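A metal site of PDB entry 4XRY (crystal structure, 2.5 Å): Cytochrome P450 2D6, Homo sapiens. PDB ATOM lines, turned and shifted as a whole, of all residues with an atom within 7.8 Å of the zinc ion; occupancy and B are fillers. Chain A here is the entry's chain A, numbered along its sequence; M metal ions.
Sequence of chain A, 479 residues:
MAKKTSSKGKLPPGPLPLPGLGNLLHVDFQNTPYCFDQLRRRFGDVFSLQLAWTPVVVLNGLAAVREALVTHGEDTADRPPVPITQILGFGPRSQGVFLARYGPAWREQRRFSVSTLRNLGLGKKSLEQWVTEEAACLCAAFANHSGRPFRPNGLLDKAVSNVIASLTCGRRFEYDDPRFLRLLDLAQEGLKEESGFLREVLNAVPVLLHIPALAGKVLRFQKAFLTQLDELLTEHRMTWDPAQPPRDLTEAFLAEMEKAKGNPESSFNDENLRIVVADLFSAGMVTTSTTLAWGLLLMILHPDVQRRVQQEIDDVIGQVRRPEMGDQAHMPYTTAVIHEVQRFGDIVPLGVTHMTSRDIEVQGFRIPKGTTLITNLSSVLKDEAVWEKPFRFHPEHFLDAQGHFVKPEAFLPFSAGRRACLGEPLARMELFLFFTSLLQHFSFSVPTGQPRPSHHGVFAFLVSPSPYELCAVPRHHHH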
ATOM      1  N   ALA A 165     -13.717  -3.257 -25.289  1.00  0.00           N
ATOM      2  CA  ALA A 165     -12.411  -2.823 -25.778  1.00  0.00           C
ATOM      3  C   ALA A 165     -12.534  -2.235 -27.176  1.00  0.00           C
ATOM      4  O   ALA A 165     -11.842  -1.273 -27.517  1.00  0.00           O
ATOM      5  CB  ALA A 165     -11.438  -3.989 -25.782  1.00  0.00           C
ATOM      6  N   SER A 166     -13.419  -2.809 -27.981  1.00  0.00           N
ATOM      7  CA  SER A 166     -13.652  -2.328 -29.340  1.00  0.00           C
ATOM      8  C   SER A 166     -14.274  -0.939 -29.323  1.00  0.00           C
ATOM      9  O   SER A 166     -13.986  -0.108 -30.174  1.00  0.00           O
ATOM     10  CB  SER A 166     -14.555  -3.296 -30.094  1.00  0.00           C
ATOM     11  OG  SER A 166     -14.069  -4.623 -29.977  1.00  0.00           O
ATOM     12  N   LEU A 167     -15.152  -0.702 -28.355  1.00  0.00           N
ATOM     13  CA  LEU A 167     -15.812   0.583 -28.241  1.00  0.00           C
ATOM     14  C   LEU A 167     -14.889   1.620 -27.629  1.00  0.00           C
ATOM     15  O   LEU A 167     -14.826   2.755 -28.086  1.00  0.00           O
ATOM     16  CB  LEU A 167     -17.105   0.462 -27.431  1.00  0.00           C
ATOM     17  CG  LEU A 167     -18.153  -0.415 -28.100  1.00  0.00           C
ATOM     18  CD1 LEU A 167     -19.516  -0.235 -27.474  1.00  0.00           C
ATOM     19  CD2 LEU A 167     -18.206  -0.100 -29.585  1.00  0.00           C
ATOM     20  N   THR A 168     -14.173   1.219 -26.577  1.00  0.00           N
ATOM     21  CA  THR A 168     -13.265   2.128 -25.894  1.00  0.00           C
ATOM     22  C   THR A 168     -11.981   2.358 -26.690  1.00  0.00           C
ATOM     23  O   THR A 168     -11.666   3.497 -27.037  1.00  0.00           O
ATOM     24  CB  THR A 168     -12.930   1.622 -24.482  1.00  0.00           C
ATOM     25  OG1 THR A 168     -12.610   0.224 -24.532  1.00  0.00           O
ATOM     26  CG2 THR A 168     -14.119   1.805 -23.557  1.00  0.00           C
ATOM     27  N   CYS A 169     -11.243   1.288 -26.986  1.00  0.00           N
ATOM     28  CA  CYS A 169      -9.926   1.449 -27.605  1.00  0.00           C
ATOM     29  C   CYS A 169      -9.861   1.036 -29.079  1.00  0.00           C
ATOM     30  O   CYS A 169      -8.800   1.095 -29.688  1.00  0.00           O
ATOM     31  CB  CYS A 169      -8.883   0.666 -26.809  1.00  0.00           C
ATOM     32  SG  CYS A 169      -8.367   1.500 -25.291  1.00  0.00           S
ATOM     33  N   GLY A 170     -10.984   0.625 -29.649  1.00  0.00           N
ATOM     34  CA  GLY A 170     -11.029   0.300 -31.064  1.00  0.00           C
ATOM     35  C   GLY A 170     -10.215  -0.916 -31.472  1.00  0.00           C
ATOM     36  O   GLY A 170      -9.748  -1.013 -32.604  1.00  0.00           O
ATOM     37  N   ARG A 171     -10.035  -1.854 -30.546  1.00  0.00           N
ATOM     38  CA  ARG A 171      -9.332  -3.093 -30.865  1.00  0.00           C
ATOM     39  C   ARG A 171      -9.959  -4.264 -30.107  1.00  0.00           C
ATOM     40  O   ARG A 171     -10.739  -4.064 -29.183  1.00  0.00           O
ATOM     41  CB  ARG A 171      -7.853  -2.988 -30.519  1.00  0.00           C
ATOM     42  CG  ARG A 171      -7.559  -3.086 -29.026  1.00  0.00           C
ATOM     43  CD  ARG A 171      -6.112  -3.454 -28.745  1.00  0.00           C
ATOM     44  NE  ARG A 171      -5.788  -4.786 -29.228  1.00  0.00           N
ATOM     45  CZ  ARG A 171      -4.614  -5.391 -29.031  1.00  0.00           C
ATOM     46  NH1 ARG A 171      -3.666  -4.779 -28.344  1.00  0.00           N
ATOM     47  NH2 ARG A 171      -4.404  -6.613 -29.508  1.00  0.00           N
ATOM     48  N   HIS A 236      -2.531   3.147 -27.080  1.00  0.00           N
ATOM     49  CA  HIS A 236      -3.634   3.664 -27.878  1.00  0.00           C
ATOM     50  C   HIS A 236      -3.401   5.131 -28.252  1.00  0.00           C
ATOM     51  O   HIS A 236      -3.744   5.563 -29.342  1.00  0.00           O
ATOM     52  CB  HIS A 236      -4.957   3.505 -27.127  1.00  0.00           C
ATOM     53  CG  HIS A 236      -6.163   3.783 -27.973  1.00  0.00           C
ATOM     54  ND1 HIS A 236      -7.415   3.985 -27.436  1.00  0.00           N
ATOM     55  CD2 HIS A 236      -6.313   3.885 -29.311  1.00  0.00           C
ATOM     56  CE1 HIS A 236      -8.277   4.204 -28.409  1.00  0.00           C
ATOM     57  NE2 HIS A 236      -7.633   4.149 -29.558  1.00  0.00           N
ATOM     58  N   ARG A 237      -2.807   5.879 -27.327  1.00  0.00           N
ATOM     59  CA  ARG A 237      -2.526   7.289 -27.551  1.00  0.00           C
ATOM     60  C   ARG A 237      -1.460   7.452 -28.640  1.00  0.00           C
ATOM     61  O   ARG A 237      -1.420   8.463 -29.339  1.00  0.00           O
ATOM     62  CB  ARG A 237      -2.071   7.972 -26.255  1.00  0.00           C
ATOM     63  CG  ARG A 237      -2.076   9.498 -26.315  1.00  0.00           C
ATOM     64  CD  ARG A 237      -1.423  10.090 -25.067  1.00  0.00           C
ATOM     65  NE  ARG A 237      -2.218   9.903 -23.866  1.00  0.00           N
ATOM     66  CZ  ARG A 237      -2.977  10.855 -23.319  1.00  0.00           C
ATOM     67  NH1 ARG A 237      -3.037  12.050 -23.882  1.00  0.00           N
ATOM     68  NH2 ARG A 237      -3.669  10.603 -22.212  1.00  0.00           N
ATOM     69  N   THR A 239      -1.107   5.300 -31.316  1.00  0.00           N
ATOM     70  CA  THR A 239      -1.644   4.940 -32.626  1.00  0.00           C
ATOM     71  C   THR A 239      -2.776   5.865 -33.060  1.00  0.00           C
ATOM     72  O   THR A 239      -3.214   5.815 -34.216  1.00  0.00           O
ATOM     73  CB  THR A 239      -2.182   3.489 -32.643  1.00  0.00           C
ATOM     74  OG1 THR A 239      -3.201   3.344 -31.658  1.00  0.00           O
ATOM     75  CG2 THR A 239      -1.054   2.494 -32.362  1.00  0.00           C
ATOM     76  N   TRP A 240      -3.244   6.704 -32.146  1.00  0.00           N
ATOM     77  CA  TRP A 240      -4.363   7.616 -32.409  1.00  0.00           C
ATOM     78  C   TRP A 240      -4.033   8.624 -33.510  1.00  0.00           C
ATOM     79  O   TRP A 240      -3.032   9.340 -33.427  1.00  0.00           O
ATOM     80  CB  TRP A 240      -4.755   8.362 -31.132  1.00  0.00           C
ATOM     81  CG  TRP A 240      -5.757   9.456 -31.348  1.00  0.00           C
ATOM     82  CD1 TRP A 240      -6.831   9.446 -32.198  1.00  0.00           C
ATOM     83  CD2 TRP A 240      -5.761  10.748 -30.723  1.00  0.00           C
ATOM     84  NE1 TRP A 240      -7.507  10.641 -32.122  1.00  0.00           N
ATOM     85  CE2 TRP A 240      -6.865  11.458 -31.233  1.00  0.00           C
ATOM     86  CE3 TRP A 240      -4.925  11.372 -29.787  1.00  0.00           C
ATOM     87  CZ2 TRP A 240      -7.168  12.760 -30.825  1.00  0.00           C
ATOM     88  CZ3 TRP A 240      -5.233  12.659 -29.385  1.00  0.00           C
ATOM     89  CH2 TRP A 240      -6.342  13.340 -29.899  1.00  0.00           C
ATOM     90  N   ASP A 241      -4.890   8.674 -34.524  1.00  0.00           N
ATOM     91  CA  ASP A 241      -4.749   9.625 -35.623  1.00  0.00           C
ATOM     92  C   ASP A 241      -5.778  10.740 -35.491  1.00  0.00           C
ATOM     93  O   ASP A 241      -6.933  10.578 -35.887  1.00  0.00           O
ATOM     94  CB  ASP A 241      -4.887   8.906 -36.967  1.00  0.00           C
ATOM     95  CG  ASP A 241      -4.667   9.826 -38.160  1.00  0.00           C
ATOM     96  OD1 ASP A 241      -4.934   9.400 -39.298  1.00  0.00           O
ATOM     97  OD2 ASP A 241      -4.238  10.982 -37.961  1.00  0.00           O
ATOM     98  N   PRO A 246     -12.727  10.493 -34.682  1.00  0.00           N
ATOM     99  CA  PRO A 246     -12.545   9.516 -33.612  1.00  0.00           C
ATOM    100  C   PRO A 246     -13.152   8.163 -33.960  1.00  0.00           C
ATOM    101  O   PRO A 246     -14.295   8.088 -34.404  1.00  0.00           O
ATOM    102  CB  PRO A 246     -13.272  10.144 -32.427  1.00  0.00           C
ATOM    103  CG  PRO A 246     -13.115  11.611 -32.666  1.00  0.00           C
ATOM    104  CD  PRO A 246     -13.153  11.805 -34.156  1.00  0.00           C
ATOM    105  N   ARG A 247     -12.373   7.103 -33.794  1.00  0.00           N
ATOM    106  CA  ARG A 247     -12.804   5.771 -34.204  1.00  0.00           C
ATOM    107  C   ARG A 247     -13.376   4.983 -33.028  1.00  0.00           C
ATOM    108  O   ARG A 247     -14.005   3.943 -33.206  1.00  0.00           O
ATOM    109  CB  ARG A 247     -11.622   5.019 -34.829  1.00  0.00           C
ATOM    110  CG  ARG A 247     -11.999   4.096 -35.970  1.00  0.00           C
ATOM    111  CD  ARG A 247     -10.778   3.347 -36.473  1.00  0.00           C
ATOM    112  NE  ARG A 247     -10.119   2.641 -35.392  1.00  0.00           N
ATOM    113  CZ  ARG A 247     -10.401   1.390 -35.040  1.00  0.00           C
ATOM    114  NH1 ARG A 247     -11.333   0.706 -35.689  1.00  0.00           N
ATOM    115  NH2 ARG A 247      -9.751   0.824 -34.039  1.00  0.00           N
ATOM    116  N   ASP A 248     -13.161   5.502 -31.826  1.00  0.00           N
ATOM    117  CA  ASP A 248     -13.580   4.842 -30.598  1.00  0.00           C
ATOM    118  C   ASP A 248     -13.722   5.862 -29.480  1.00  0.00           C
ATOM    119  O   ASP A 248     -13.325   7.021 -29.639  1.00  0.00           O
ATOM    120  CB  ASP A 248     -12.583   3.739 -30.223  1.00  0.00           C
ATOM    121  CG  ASP A 248     -11.133   4.221 -30.271  1.00  0.00           C
ATOM    122  OD1 ASP A 248     -10.798   5.182 -29.550  1.00  0.00           O
ATOM    123  OD2 ASP A 248     -10.339   3.629 -31.030  1.00  0.00           O
ATOM    124  N   LEU A 249     -14.287   5.456 -28.345  1.00  0.00           N
ATOM    125  CA  LEU A 249     -14.613   6.391 -27.276  1.00  0.00           C
ATOM    126  C   LEU A 249     -13.383   7.073 -26.690  1.00  0.00           C
ATOM    127  O   LEU A 249     -13.423   8.249 -26.350  1.00  0.00           O
ATOM    128  CB  LEU A 249     -15.399   5.680 -26.164  1.00  0.00           C
ATOM    129  CG  LEU A 249     -15.853   6.579 -25.003  1.00  0.00           C
ATOM    130  CD1 LEU A 249     -17.311   6.340 -24.670  1.00  0.00           C
ATOM    131  CD2 LEU A 249     -14.987   6.379 -23.769  1.00  0.00           C
ATOM    132  N   THR A 250     -12.288   6.325 -26.588  1.00  0.00           N
ATOM    133  CA  THR A 250     -11.048   6.881 -26.040  1.00  0.00           C
ATOM    134  C   THR A 250     -10.506   7.994 -26.939  1.00  0.00           C
ATOM    135  O   THR A 250      -9.996   9.006 -26.437  1.00  0.00           O
ATOM    136  CB  THR A 250      -9.978   5.777 -25.862  1.00  0.00           C
ATOM    137  OG1 THR A 250     -10.396   4.879 -24.825  1.00  0.00           O
ATOM    138  CG2 THR A 250      -8.626   6.380 -25.485  1.00  0.00           C
ATOM    139  N   GLU A 251     -10.622   7.837 -28.250  1.00  0.00           N
ATOM    140  CA  GLU A 251     -10.176   8.872 -29.177  1.00  0.00           C
ATOM    141  C   GLU A 251     -11.065  10.101 -29.044  1.00  0.00           C
ATOM    142  O   GLU A 251     -10.575  11.240 -29.055  1.00  0.00           O
ATOM    143  CB  GLU A 251     -10.175   8.362 -30.610  1.00  0.00           C
ATOM    144  CG  GLU A 251      -9.058   7.364 -30.905  1.00  0.00           C
ATOM    145  CD  GLU A 251      -9.101   6.840 -32.327  1.00  0.00           C
ATOM    146  OE1 GLU A 251      -9.754   7.483 -33.173  1.00  0.00           O
ATOM    147  OE2 GLU A 251      -8.496   5.783 -32.587  1.00  0.00           O
ATOM    148  N   ALA A 252     -12.370   9.877 -28.920  1.00  0.00           N
ATOM    149  CA  ALA A 252     -13.315  10.962 -28.721  1.00  0.00           C
ATOM    150  C   ALA A 252     -12.996  11.717 -27.433  1.00  0.00           C
ATOM    151  O   ALA A 252     -13.061  12.949 -27.375  1.00  0.00           O
ATOM    152  CB  ALA A 252     -14.740  10.437 -28.685  1.00  0.00           C
ATOM    153  N   LEU A 254      -9.987  11.828 -25.964  1.00  0.00           N
ATOM    154  CA  LEU A 254      -8.707  12.513 -26.155  1.00  0.00           C
ATOM    155  C   LEU A 254      -8.866  13.812 -26.938  1.00  0.00           C
ATOM    156  O   LEU A 254      -8.196  14.804 -26.645  1.00  0.00           O
ATOM    157  CB  LEU A 254      -7.707  11.586 -26.866  1.00  0.00           C
ATOM    158  CG  LEU A 254      -7.193  10.380 -26.078  1.00  0.00           C
ATOM    159  CD1 LEU A 254      -6.551   9.361 -27.008  1.00  0.00           C
ATOM    160  CD2 LEU A 254      -6.216  10.801 -24.989  1.00  0.00           C
HETATM  161 ZN    ZN M   1      -8.474   4.209 -31.451  1.00  0.00          ZN
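The side-chain hydroxyl (OG1) of Thr 239 lies within hydrogen-bond range of the backbone carbonyl oxygen (O) of His 236, at 3.3 Å. O of Cys 169 sits close to NE2 of His 236 (3.3 Å). The backbone NH (N) of Arg 247 sits at hydrogen-bond distance from the side-chain carboxylate (OE1) of Glu 251, at 2.7 Å. The side-chain carboxylate (OD2) of Asp 248 sits close to the backbone NH (N) of Gly 170.
Merely in contact with the zinc ion: Cys 169 (3.6 Å). Within 4 Å of the zinc ion: Cys 169, His 236, Asp 248 and Glu 251.
The zinc ion is bound by the side-chain carboxylate (OE2) of Glu 251 (1.9 Å), the side-chain carboxylate (OD2) of Asp 248 (2.0 Å) and a ring nitrogen (NE2) of His 236 (2.1 Å). The zinc ion has three donor atoms within binding distance.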
